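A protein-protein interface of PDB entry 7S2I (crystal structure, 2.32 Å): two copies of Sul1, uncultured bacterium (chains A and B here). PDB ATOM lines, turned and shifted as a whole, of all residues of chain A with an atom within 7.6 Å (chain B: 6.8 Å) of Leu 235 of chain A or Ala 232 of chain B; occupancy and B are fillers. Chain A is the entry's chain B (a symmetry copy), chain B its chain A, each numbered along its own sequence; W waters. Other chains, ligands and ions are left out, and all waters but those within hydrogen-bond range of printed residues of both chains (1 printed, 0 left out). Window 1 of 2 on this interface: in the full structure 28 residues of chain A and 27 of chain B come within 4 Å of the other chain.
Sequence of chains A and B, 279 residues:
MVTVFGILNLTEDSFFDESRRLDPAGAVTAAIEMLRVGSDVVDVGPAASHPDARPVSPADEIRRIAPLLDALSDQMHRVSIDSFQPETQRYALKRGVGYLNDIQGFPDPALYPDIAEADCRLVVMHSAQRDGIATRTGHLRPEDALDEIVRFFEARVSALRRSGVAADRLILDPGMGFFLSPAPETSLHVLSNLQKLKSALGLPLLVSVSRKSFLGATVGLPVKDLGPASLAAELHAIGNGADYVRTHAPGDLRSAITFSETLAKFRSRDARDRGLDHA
The backbone carbonyl oxygen (O) of Asp 252 of chain A lies within hydrogen-bond range of the side-chain hydroxyl (OG) of Ser 255 of chain A. O of Ala 256 of chain A lies within hydrogen-bond range of OG of Ser 260 of chain A (3.0 Å).
Leu 231 of chain B touches Pro 228 of chain A. O of Pro 228 of chain B touches CD2 of Leu 231 of chain A, at 3.7 Å. Ala 232 of chain A touches Leu 235 of chain B (CB to CD1, 3.96 Å). Ala 232 of chain B touches Leu 235 of chain A. Asp 252 of chain A touches Pro 228 of chain B. Ser 255 of chain A touches Ala 229 of chain B (OG to N, 3.9 Å). Ala 232 of chain B touches Ala 256 of chain A (CB to CB, 3.9 Å). Leu 191 of chain B touches Phe 259 of chain A (CD2 to CZ, 3.8 Å). Ala 233 of chain B touches Phe 259 of chain A (CA to CE2, 3.5 Å). CD2 of Leu 263 of chain A touches CD2 of His 236 of chain B (3.3 Å).
Pro 228 of chain A touches Leu 231 of chain B, and with the chains exchanged Leu 231 of chain A touches Pro 228 of chain B. Ala 232 of chain A touches Leu 235 of chain B, and with the chains exchanged Leu 235 of chain A touches Ala 232 of chain B. Positions printed for both chains: 191, 209, 228, 229, 230, 231, 232, 233, 234, 235, 236 and 237. Of the 11 pairs that touch across the chains among the printed residues, 4 have their exchanged pair printed and touching as well.
Water W1 lies within hydrogen-bond range of the side-chain hydroxyl of Ser 255 of chain A (2.5 Å) and the backbone NH of Ala 229 of chain B (2.9 Å).
Of the 14 printed residues of chain B, 8 touch a printed residue of chain A. Printed residues of chain B that touch a printed residue of chain A: Leu 191, Pro 228, Ala 229, Leu 231, Ala 232, Ala 233, Leu 235 and His 236. Along chain B the printed residues that touch a printed residue of chain A span positions 191 to 236. Printed residues of chain A that touch a printed residue of chain B: Pro 228, Leu 231, Ala 232, Leu 235, Asp 252, Ser 255, Ala 256, Phe 259 and Leu 263. Among the printed residues, no Asp or Glu carboxylate lies within 4 Å of a Lys or Arg side-chain nitrogen of the other chain.
Leu 191 of chain A touches none of the printed residues of chain B. Of the printed residues of chain B, Leu 231 of chain A touches Pro 228. Leu 235 of chain A touches one residue of chain B. Of the printed residues of chain B, Ala 256 of chain A touches Ala 232 (3.9 Å). Ala 232 of chain B touches just these residues of chain A: Leu 235 and Ala 256. Of the printed residues of chain A, His 236 of chain B touches Leu 263. The nearest residue of chain B that does not touch Leu 235 of chain A is Leu 235 of chain B (4.7 Å).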
ATOM      1  N   LEU A 191      10.206 -18.258  15.166  1.00  0.00           N
ATOM      2  CA  LEU A 191       9.312 -17.158  14.821  1.00  0.00           C
ATOM      3  C   LEU A 191       7.884 -17.451  15.263  1.00  0.00           C
ATOM      4  O   LEU A 191       7.220 -16.596  15.864  1.00  0.00           O
ATOM      5  CB  LEU A 191       9.372 -16.896  13.317  1.00  0.00           C
ATOM      6  CG  LEU A 191       8.472 -15.783  12.796  1.00  0.00           C
ATOM      7  CD1 LEU A 191       8.901 -14.468  13.410  1.00  0.00           C
ATOM      8  CD2 LEU A 191       8.557 -15.723  11.286  1.00  0.00           C
ATOM      9  N   VAL A 209      13.924 -10.913   9.539  1.00  0.00           N
ATOM     10  CA  VAL A 209      13.572 -12.043   8.687  1.00  0.00           C
ATOM     11  C   VAL A 209      13.694 -11.723   7.201  1.00  0.00           C
ATOM     12  O   VAL A 209      13.725 -12.656   6.382  1.00  0.00           O
ATOM     13  CB  VAL A 209      12.142 -12.538   8.993  1.00  0.00           C
ATOM     14  CG1 VAL A 209      12.029 -12.968  10.452  1.00  0.00           C
ATOM     15  CG2 VAL A 209      11.136 -11.449   8.676  1.00  0.00           C
ATOM     16  N   PRO A 228       6.816  -9.756  -0.339  1.00  0.00           N
ATOM     17  CA  PRO A 228       5.543 -10.098   0.329  1.00  0.00           C
ATOM     18  C   PRO A 228       5.684 -11.099   1.466  1.00  0.00           C
ATOM     19  O   PRO A 228       5.146 -10.859   2.555  1.00  0.00           O
ATOM     20  CB  PRO A 228       4.688 -10.644  -0.826  1.00  0.00           C
ATOM     21  CG  PRO A 228       5.233  -9.958  -2.049  1.00  0.00           C
ATOM     22  CD  PRO A 228       6.716  -9.850  -1.809  1.00  0.00           C
ATOM     23  N   ALA A 229       6.376 -12.225   1.244  1.00  0.00           N
ATOM     24  CA  ALA A 229       6.571 -13.194   2.323  1.00  0.00           C
ATOM     25  C   ALA A 229       7.266 -12.553   3.517  1.00  0.00           C
ATOM     26  O   ALA A 229       6.920 -12.834   4.673  1.00  0.00           O
ATOM     27  CB  ALA A 229       7.373 -14.396   1.823  1.00  0.00           C
ATOM     28  N   SER A 230       8.241 -11.680   3.258  1.00  0.00           N
ATOM     29  CA  SER A 230       8.926 -10.987   4.346  1.00  0.00           C
ATOM     30  C   SER A 230       7.966 -10.110   5.131  1.00  0.00           C
ATOM     31  O   SER A 230       7.998 -10.091   6.367  1.00  0.00           O
ATOM     32  CB  SER A 230      10.082 -10.144   3.798  1.00  0.00           C
ATOM     33  OG  SER A 230      11.017 -10.940   3.077  1.00  0.00           O
ATOM     34  N   LEU A 231       7.114  -9.367   4.430  1.00  0.00           N
ATOM     35  CA  LEU A 231       6.159  -8.512   5.117  1.00  0.00           C
ATOM     36  C   LEU A 231       5.229  -9.340   6.003  1.00  0.00           C
ATOM     37  O   LEU A 231       4.974  -8.979   7.161  1.00  0.00           O
ATOM     38  CB  LEU A 231       5.375  -7.697   4.089  1.00  0.00           C
ATOM     39  CG  LEU A 231       4.513  -6.564   4.640  1.00  0.00           C
ATOM     40  CD1 LEU A 231       5.397  -5.496   5.265  1.00  0.00           C
ATOM     41  CD2 LEU A 231       3.628  -5.971   3.547  1.00  0.00           C
ATOM     42  N   ALA A 232       4.742 -10.474   5.488  1.00  0.00           N
ATOM     43  CA  ALA A 232       3.906 -11.360   6.294  1.00  0.00           C
ATOM     44  C   ALA A 232       4.647 -11.841   7.532  1.00  0.00           C
ATOM     45  O   ALA A 232       4.104 -11.804   8.644  1.00  0.00           O
ATOM     46  CB  ALA A 232       3.450 -12.556   5.458  1.00  0.00           C
ATOM     47  N   ALA A 233       5.886 -12.310   7.351  1.00  0.00           N
ATOM     48  CA  ALA A 233       6.700 -12.747   8.479  1.00  0.00           C
ATOM     49  C   ALA A 233       6.881 -11.625   9.488  1.00  0.00           C
ATOM     50  O   ALA A 233       6.757 -11.842  10.699  1.00  0.00           O
ATOM     51  CB  ALA A 233       8.060 -13.232   7.979  1.00  0.00           C
ATOM     52  N   GLU A 234       7.181 -10.418   8.996  1.00  0.00           N
ATOM     53  CA  GLU A 234       7.385  -9.260   9.863  1.00  0.00           C
ATOM     54  C   GLU A 234       6.128  -8.929  10.664  1.00  0.00           C
ATOM     55  O   GLU A 234       6.202  -8.667  11.871  1.00  0.00           O
ATOM     56  CB  GLU A 234       7.807  -8.050   9.024  1.00  0.00           C
ATOM     57  CG  GLU A 234       9.308  -7.894   8.725  1.00  0.00           C
ATOM     58  CD  GLU A 234       9.610  -7.240   7.379  1.00  0.00           C
ATOM     59  OE1 GLU A 234      10.655  -7.569   6.761  1.00  0.00           O
ATOM     60  OE2 GLU A 234       8.758  -6.447   6.905  1.00  0.00           O
ATOM     61  N   LEU A 235       4.966  -8.932  10.011  1.00  0.00           N
ATOM     62  CA  LEU A 235       3.721  -8.610  10.706  1.00  0.00           C
ATOM     63  C   LEU A 235       3.386  -9.637  11.777  1.00  0.00           C
ATOM     64  O   LEU A 235       2.818  -9.283  12.820  1.00  0.00           O
ATOM     65  CB  LEU A 235       2.576  -8.506   9.700  1.00  0.00           C
ATOM     66  CG  LEU A 235       2.675  -7.284   8.781  1.00  0.00           C
ATOM     67  CD1 LEU A 235       1.617  -7.336   7.686  1.00  0.00           C
ATOM     68  CD2 LEU A 235       2.535  -6.018   9.615  1.00  0.00           C
ATOM     69  N   HIS A 236       3.715 -10.909  11.539  1.00  0.00           N
ATOM     70  CA  HIS A 236       3.543 -11.903  12.592  1.00  0.00           C
ATOM     71  C   HIS A 236       4.489 -11.636  13.754  1.00  0.00           C
ATOM     72  O   HIS A 236       4.083 -11.708  14.921  1.00  0.00           O
ATOM     73  CB  HIS A 236       3.744 -13.317  12.032  1.00  0.00           C
ATOM     74  CG  HIS A 236       3.729 -14.396  13.079  1.00  0.00           C
ATOM     75  ND1 HIS A 236       4.615 -14.437  14.137  1.00  0.00           N
ATOM     76  CD2 HIS A 236       2.866 -15.422  13.278  1.00  0.00           C
ATOM     77  CE1 HIS A 236       4.333 -15.472  14.910  1.00  0.00           C
ATOM     78  NE2 HIS A 236       3.274 -16.085  14.412  1.00  0.00           N
ATOM     79  N   ALA A 237       5.754 -11.337  13.455  1.00  0.00           N
ATOM     80  CA  ALA A 237       6.719 -11.089  14.520  1.00  0.00           C
ATOM     81  C   ALA A 237       6.263  -9.943  15.413  1.00  0.00           C
ATOM     82  O   ALA A 237       6.335 -10.033  16.646  1.00  0.00           O
ATOM     83  CB  ALA A 237       8.094 -10.786  13.919  1.00  0.00           C
ATOM     84  N   ILE A 238       5.765  -8.867  14.797  1.00  0.00           N
ATOM     85  CA  ILE A 238       5.284  -7.698  15.528  1.00  0.00           C
ATOM     86  C   ILE A 238       4.116  -8.069  16.432  1.00  0.00           C
ATOM     87  O   ILE A 238       4.023  -7.604  17.576  1.00  0.00           O
ATOM     88  CB  ILE A 238       4.901  -6.596  14.525  1.00  0.00           C
ATOM     89  CG1 ILE A 238       6.145  -6.141  13.754  1.00  0.00           C
ATOM     90  CG2 ILE A 238       4.154  -5.465  15.220  1.00  0.00           C
ATOM     91  CD1 ILE A 238       6.049  -4.752  13.215  1.00  0.00           C
ATOM     92  N   GLY A 239       3.207  -8.903  15.937  1.00  0.00           N
ATOM     93  CA  GLY A 239       2.118  -9.369  16.768  1.00  0.00           C
ATOM     94  C   GLY A 239       2.523 -10.361  17.834  1.00  0.00           C
ATOM     95  O   GLY A 239       1.681 -10.750  18.646  1.00  0.00           O
ATOM     96  N   ASN A 240       3.786 -10.784  17.857  1.00  0.00           N
ATOM     97  CA  ASN A 240       4.234 -11.791  18.811  1.00  0.00           C
ATOM     98  C   ASN A 240       5.431 -11.303  19.616  1.00  0.00           C
ATOM     99  O   ASN A 240       6.289 -12.101  20.003  1.00  0.00           O
ATOM    100  CB  ASN A 240       4.551 -13.106  18.100  1.00  0.00           C
ATOM    101  CG  ASN A 240       3.303 -13.882  17.756  1.00  0.00           C
ATOM    102  OD1 ASN A 240       2.965 -14.867  18.412  1.00  0.00           O
ATOM    103  ND2 ASN A 240       2.588 -13.422  16.738  1.00  0.00           N
ATOM    104  N   GLY A 241       5.514  -9.993  19.853  1.00  0.00           N
ATOM    105  CA  GLY A 241       6.452  -9.435  20.808  1.00  0.00           C
ATOM    106  C   GLY A 241       7.660  -8.722  20.239  1.00  0.00           C
ATOM    107  O   GLY A 241       8.455  -8.188  21.021  1.00  0.00           O
ATOM    108  N   VAL A 245      12.212  -4.256  14.133  1.00  0.00           N
ATOM    109  CA  VAL A 245      12.285  -5.084  12.934  1.00  0.00           C
ATOM    110  C   VAL A 245      13.306  -4.488  11.974  1.00  0.00           C
ATOM    111  O   VAL A 245      13.252  -3.294  11.658  1.00  0.00           O
ATOM    112  CB  VAL A 245      10.921  -5.226  12.236  1.00  0.00           C
ATOM    113  CG1 VAL A 245      11.086  -6.107  11.014  1.00  0.00           C
ATOM    114  CG2 VAL A 245       9.870  -5.811  13.199  1.00  0.00           C
ATOM    115  N   ASP A 252       7.638   0.182   3.202  1.00  0.00           N
ATOM    116  CA  ASP A 252       6.548  -0.787   3.094  1.00  0.00           C
ATOM    117  C   ASP A 252       6.074  -1.228   4.471  1.00  0.00           C
ATOM    118  O   ASP A 252       4.877  -1.173   4.773  1.00  0.00           O
ATOM    119  CB  ASP A 252       6.995  -2.004   2.278  1.00  0.00           C
ATOM    120  CG  ASP A 252       7.275  -1.663   0.818  1.00  0.00           C
ATOM    121  OD1 ASP A 252       7.006  -0.511   0.402  1.00  0.00           O
ATOM    122  OD2 ASP A 252       7.751  -2.557   0.083  1.00  0.00           O
ATOM    123  N   LEU A 253       7.013  -1.659   5.325  1.00  0.00           N
ATOM    124  CA  LEU A 253       6.647  -2.192   6.632  1.00  0.00           C
ATOM    125  C   LEU A 253       5.965  -1.137   7.493  1.00  0.00           C
ATOM    126  O   LEU A 253       4.931  -1.411   8.116  1.00  0.00           O
ATOM    127  CB  LEU A 253       7.884  -2.753   7.339  1.00  0.00           C
ATOM    128  CG  LEU A 253       7.663  -3.226   8.775  1.00  0.00           C
ATOM    129  CD1 LEU A 253       6.573  -4.281   8.820  1.00  0.00           C
ATOM    130  CD2 LEU A 253       8.956  -3.769   9.349  1.00  0.00           C
ATOM    131  N   ARG A 254       6.512   0.081   7.528  1.00  0.00           N
ATOM    132  CA  ARG A 254       5.890   1.129   8.330  1.00  0.00           C
ATOM    133  C   ARG A 254       4.461   1.388   7.874  1.00  0.00           C
ATOM    134  O   ARG A 254       3.571   1.611   8.702  1.00  0.00           O
ATOM    135  CB  ARG A 254       6.716   2.417   8.275  1.00  0.00           C
ATOM    136  CG  ARG A 254       5.998   3.649   8.864  1.00  0.00           C
ATOM    137  CD  ARG A 254       5.587   3.430  10.326  1.00  0.00           C
ATOM    138  NE  ARG A 254       6.735   3.239  11.204  1.00  0.00           N
ATOM    139  CZ  ARG A 254       6.674   2.703  12.415  1.00  0.00           C
ATOM    140  NH1 ARG A 254       5.531   2.276  12.925  1.00  0.00           N
ATOM    141  NH2 ARG A 254       7.789   2.594  13.135  1.00  0.00           N
ATOM    142  N   SER A 255       4.211   1.335   6.563  1.00  0.00           N
ATOM    143  CA  SER A 255       2.855   1.574   6.083  1.00  0.00           C
ATOM    144  C   SER A 255       1.919   0.433   6.480  1.00  0.00           C
ATOM    145  O   SER A 255       0.754   0.672   6.817  1.00  0.00           O
ATOM    146  CB  SER A 255       2.867   1.809   4.566  1.00  0.00           C
ATOM    147  OG  SER A 255       2.728   0.606   3.819  1.00  0.00           O
ATOM    148  N   ALA A 256       2.413  -0.811   6.491  1.00  0.00           N
ATOM    149  CA  ALA A 256       1.577  -1.913   6.964  1.00  0.00           C
ATOM    150  C   ALA A 256       1.344  -1.827   8.471  1.00  0.00           C
ATOM    151  O   ALA A 256       0.251  -2.152   8.952  1.00  0.00           O
ATOM    152  CB  ALA A 256       2.199  -3.259   6.592  1.00  0.00           C
ATOM    153  N   ILE A 257       2.353  -1.387   9.233  1.00  0.00           N
ATOM    154  CA  ILE A 257       2.175  -1.249  10.679  1.00  0.00           C
ATOM    155  C   ILE A 257       1.132  -0.185  10.980  1.00  0.00           C
ATOM    156  O   ILE A 257       0.219  -0.395  11.789  1.00  0.00           O
ATOM    157  CB  ILE A 257       3.506  -0.918  11.375  1.00  0.00           C
ATOM    158  CG1 ILE A 257       4.490  -2.076  11.261  1.00  0.00           C
ATOM    159  CG2 ILE A 257       3.248  -0.582  12.853  1.00  0.00           C
ATOM    160  CD1 ILE A 257       5.913  -1.661  11.610  1.00  0.00           C
ATOM    161  N   THR A 258       1.254   0.979  10.330  1.00  0.00           N
ATOM    162  CA  THR A 258       0.256   2.028  10.513  1.00  0.00           C
ATOM    163  C   THR A 258      -1.146   1.509  10.218  1.00  0.00           C
ATOM    164  O   THR A 258      -2.094   1.816  10.951  1.00  0.00           O
ATOM    165  CB  THR A 258       0.576   3.230   9.630  1.00  0.00           C
ATOM    166  OG1 THR A 258       1.765   3.866  10.111  1.00  0.00           O
ATOM    167  CG2 THR A 258      -0.577   4.229   9.656  1.00  0.00           C
ATOM    168  N   PHE A 259      -1.298   0.704   9.163  1.00  0.00           N
ATOM    169  CA  PHE A 259      -2.622   0.169   8.867  1.00  0.00           C
ATOM    170  C   PHE A 259      -3.074  -0.808   9.942  1.00  0.00           C
ATOM    171  O   PHE A 259      -4.239  -0.795  10.350  1.00  0.00           O
ATOM    172  CB  PHE A 259      -2.655  -0.525   7.509  1.00  0.00           C
ATOM    173  CG  PHE A 259      -3.939  -1.256   7.266  1.00  0.00           C
ATOM    174  CD1 PHE A 259      -5.066  -0.570   6.842  1.00  0.00           C
ATOM    175  CD2 PHE A 259      -4.043  -2.614   7.521  1.00  0.00           C
ATOM    176  CE1 PHE A 259      -6.278  -1.232   6.644  1.00  0.00           C
ATOM    177  CE2 PHE A 259      -5.250  -3.281   7.329  1.00  0.00           C
ATOM    178  CZ  PHE A 259      -6.362  -2.591   6.885  1.00  0.00           C
ATOM    179  N   SER A 260      -2.166  -1.669  10.401  1.00  0.00           N
ATOM    180  CA  SER A 260      -2.516  -2.663  11.411  1.00  0.00           C
ATOM    181  C   SER A 260      -2.914  -1.990  12.718  1.00  0.00           C
ATOM    182  O   SER A 260      -3.939  -2.331  13.323  1.00  0.00           O
ATOM    183  CB  SER A 260      -1.335  -3.605  11.628  1.00  0.00           C
ATOM    184  OG  SER A 260      -1.096  -4.380  10.467  1.00  0.00           O
ATOM    185  N   LEU A 263      -6.270  -0.416  12.325  1.00  0.00           N
ATOM    186  CA  LEU A 263      -7.338  -1.407  12.268  1.00  0.00           C
ATOM    187  C   LEU A 263      -7.675  -1.946  13.654  1.00  0.00           C
ATOM    188  O   LEU A 263      -8.853  -2.128  13.987  1.00  0.00           O
ATOM    189  CB  LEU A 263      -6.926  -2.535  11.331  1.00  0.00           C
ATOM    190  CG  LEU A 263      -8.002  -3.505  10.878  1.00  0.00           C
ATOM    191  CD1 LEU A 263      -9.143  -2.760  10.207  1.00  0.00           C
ATOM    192  CD2 LEU A 263      -7.351  -4.458   9.910  1.00  0.00           C
ATOM    193  N   LEU B 191     -14.007  -4.264   8.033  1.00  0.00           N
ATOM    194  CA  LEU B 191     -12.872  -5.174   7.880  1.00  0.00           C
ATOM    195  C   LEU B 191     -12.417  -5.721   9.229  1.00  0.00           C
ATOM    196  O   LEU B 191     -12.248  -6.936   9.390  1.00  0.00           O
ATOM    197  CB  LEU B 191     -11.724  -4.464   7.158  1.00  0.00           C
ATOM    198  CG  LEU B 191     -10.473  -5.280   6.818  1.00  0.00           C
ATOM    199  CD1 LEU B 191     -10.801  -6.581   6.107  1.00  0.00           C
ATOM    200  CD2 LEU B 191      -9.525  -4.449   5.982  1.00  0.00           C
ATOM    201  N   VAL B 209      -9.931  -5.268  -1.107  1.00  0.00           N
ATOM    202  CA  VAL B 209      -9.425  -4.048  -0.487  1.00  0.00           C
ATOM    203  C   VAL B 209      -8.322  -3.401  -1.299  1.00  0.00           C
ATOM    204  O   VAL B 209      -8.013  -2.218  -1.069  1.00  0.00           O
ATOM    205  CB  VAL B 209      -8.890  -4.323   0.932  1.00  0.00           C
ATOM    206  CG1 VAL B 209     -10.003  -4.786   1.838  1.00  0.00           C
ATOM    207  CG2 VAL B 209      -7.770  -5.356   0.858  1.00  0.00           C
ATOM    208  N   LEU B 226       0.302   1.450  -2.291  1.00  0.00           N
ATOM    209  CA  LEU B 226      -0.584   0.777  -1.354  1.00  0.00           C
ATOM    210  C   LEU B 226      -0.465  -0.736  -1.407  1.00  0.00           C
ATOM    211  O   LEU B 226      -1.220  -1.420  -0.707  1.00  0.00           O
ATOM    212  CB  LEU B 226      -2.041   1.189  -1.606  1.00  0.00           C
ATOM    213  CG  LEU B 226      -2.377   2.661  -1.342  1.00  0.00           C
ATOM    214  CD1 LEU B 226      -3.840   2.941  -1.653  1.00  0.00           C
ATOM    215  CD2 LEU B 226      -2.046   3.047   0.092  1.00  0.00           C
ATOM    216  N   GLY B 227       0.460  -1.272  -2.209  1.00  0.00           N
ATOM    217  CA  GLY B 227       0.732  -2.694  -2.222  1.00  0.00           C
ATOM    218  C   GLY B 227       0.888  -3.294  -0.829  1.00  0.00           C
ATOM    219  O   GLY B 227       0.220  -4.268  -0.477  1.00  0.00           O
ATOM    220  N   PRO B 228       1.777  -2.724  -0.008  1.00  0.00           N
ATOM    221  CA  PRO B 228       1.992  -3.288   1.338  1.00  0.00           C
ATOM    222  C   PRO B 228       0.799  -3.153   2.266  1.00  0.00           C
ATOM    223  O   PRO B 228       0.449  -4.116   2.959  1.00  0.00           O
ATOM    224  CB  PRO B 228       3.196  -2.496   1.864  1.00  0.00           C
ATOM    225  CG  PRO B 228       3.942  -2.068   0.589  1.00  0.00           C
ATOM    226  CD  PRO B 228       2.840  -1.774  -0.394  1.00  0.00           C
ATOM    227  N   ALA B 229       0.180  -1.970   2.320  1.00  0.00           N
ATOM    228  CA  ALA B 229      -1.026  -1.821   3.132  1.00  0.00           C
ATOM    229  C   ALA B 229      -2.120  -2.776   2.659  1.00  0.00           C
ATOM    230  O   ALA B 229      -2.815  -3.387   3.480  1.00  0.00           O
ATOM    231  CB  ALA B 229      -1.517  -0.372   3.103  1.00  0.00           C
ATOM    232  N   SER B 230      -2.264  -2.942   1.341  1.00  0.00           N
ATOM    233  CA  SER B 230      -3.242  -3.897   0.819  1.00  0.00           C
ATOM    234  C   SER B 230      -2.948  -5.310   1.300  1.00  0.00           C
ATOM    235  O   SER B 230      -3.850  -6.012   1.772  1.00  0.00           O
ATOM    236  CB  SER B 230      -3.267  -3.860  -0.708  1.00  0.00           C
ATOM    237  OG  SER B 230      -3.572  -2.560  -1.180  1.00  0.00           O
ATOM    238  N   LEU B 231      -1.692  -5.745   1.191  1.00  0.00           N
ATOM    239  CA  LEU B 231      -1.333  -7.080   1.662  1.00  0.00           C
ATOM    240  C   LEU B 231      -1.671  -7.255   3.141  1.00  0.00           C
ATOM    241  O   LEU B 231      -2.258  -8.270   3.540  1.00  0.00           O
ATOM    242  CB  LEU B 231       0.151  -7.346   1.399  1.00  0.00           C
ATOM    243  CG  LEU B 231       0.612  -8.805   1.491  1.00  0.00           C
ATOM    244  CD1 LEU B 231      -0.122  -9.662   0.480  1.00  0.00           C
ATOM    245  CD2 LEU B 231       2.112  -8.906   1.269  1.00  0.00           C
ATOM    246  N   ALA B 232      -1.338  -6.263   3.969  1.00  0.00           N
ATOM    247  CA  ALA B 232      -1.707  -6.338   5.381  1.00  0.00           C
ATOM    248  C   ALA B 232      -3.218  -6.471   5.547  1.00  0.00           C
ATOM    249  O   ALA B 232      -3.695  -7.295   6.338  1.00  0.00           O
ATOM    250  CB  ALA B 232      -1.193  -5.103   6.123  1.00  0.00           C
ATOM    251  N   ALA B 233      -3.982  -5.673   4.796  1.00  0.00           N
ATOM    252  CA  ALA B 233      -5.440  -5.736   4.869  1.00  0.00           C
ATOM    253  C   ALA B 233      -5.957  -7.100   4.434  1.00  0.00           C
ATOM    254  O   ALA B 233      -6.857  -7.665   5.069  1.00  0.00           O
ATOM    255  CB  ALA B 233      -6.047  -4.632   3.999  1.00  0.00           C
ATOM    256  N   GLU B 234      -5.391  -7.648   3.358  1.00  0.00           N
ATOM    257  CA  GLU B 234      -5.846  -8.934   2.836  1.00  0.00           C
ATOM    258  C   GLU B 234      -5.578 -10.059   3.831  1.00  0.00           C
ATOM    259  O   GLU B 234      -6.456 -10.887   4.105  1.00  0.00           O
ATOM    260  CB  GLU B 234      -5.162  -9.215   1.493  1.00  0.00           C
ATOM    261  CG  GLU B 234      -5.676  -8.345   0.338  1.00  0.00           C
ATOM    262  CD  GLU B 234      -4.657  -8.158  -0.787  1.00  0.00           C
ATOM    263  OE1 GLU B 234      -3.551  -8.746  -0.706  1.00  0.00           O
ATOM    264  OE2 GLU B 234      -4.971  -7.434  -1.765  1.00  0.00           O
ATOM    265  N   LEU B 235      -4.360 -10.106   4.381  1.00  0.00           N
ATOM    266  CA  LEU B 235      -4.007 -11.144   5.346  1.00  0.00           C
ATOM    267  C   LEU B 235      -4.901 -11.069   6.567  1.00  0.00           C
ATOM    268  O   LEU B 235      -5.294 -12.097   7.134  1.00  0.00           O
ATOM    269  CB  LEU B 235      -2.540 -10.998   5.766  1.00  0.00           C
ATOM    270  CG  LEU B 235      -1.497 -11.294   4.687  1.00  0.00           C
ATOM    271  CD1 LEU B 235      -0.123 -10.884   5.171  1.00  0.00           C
ATOM    272  CD2 LEU B 235      -1.520 -12.779   4.326  1.00  0.00           C
ATOM    273  N   HIS B 236      -5.221  -9.848   6.993  1.00  0.00           N
ATOM    274  CA  HIS B 236      -6.176  -9.676   8.078  1.00  0.00           C
ATOM    275  C   HIS B 236      -7.548 -10.208   7.683  1.00  0.00           C
ATOM    276  O   HIS B 236      -8.176 -10.941   8.452  1.00  0.00           O
ATOM    277  CB  HIS B 236      -6.211  -8.196   8.477  1.00  0.00           C
ATOM    278  CG  HIS B 236      -7.098  -7.890   9.644  1.00  0.00           C
ATOM    279  ND1 HIS B 236      -8.473  -7.973   9.590  1.00  0.00           N
ATOM    280  CD2 HIS B 236      -6.791  -7.584  10.926  1.00  0.00           C
ATOM    281  CE1 HIS B 236      -8.975  -7.657  10.770  1.00  0.00           C
ATOM    282  NE2 HIS B 236      -7.975  -7.440  11.605  1.00  0.00           N
ATOM    283  N   ALA B 237      -7.998  -9.905   6.464  1.00  0.00           N
ATOM    284  CA  ALA B 237      -9.301 -10.395   6.026  1.00  0.00           C
ATOM    285  C   ALA B 237      -9.324 -11.916   5.963  1.00  0.00           C
ATOM    286  O   ALA B 237     -10.305 -12.544   6.379  1.00  0.00           O
ATOM    287  CB  ALA B 237      -9.670  -9.797   4.668  1.00  0.00           C
HETATM  288  O   HOH W   1       1.268   0.701   1.732  1.00  0.00           O
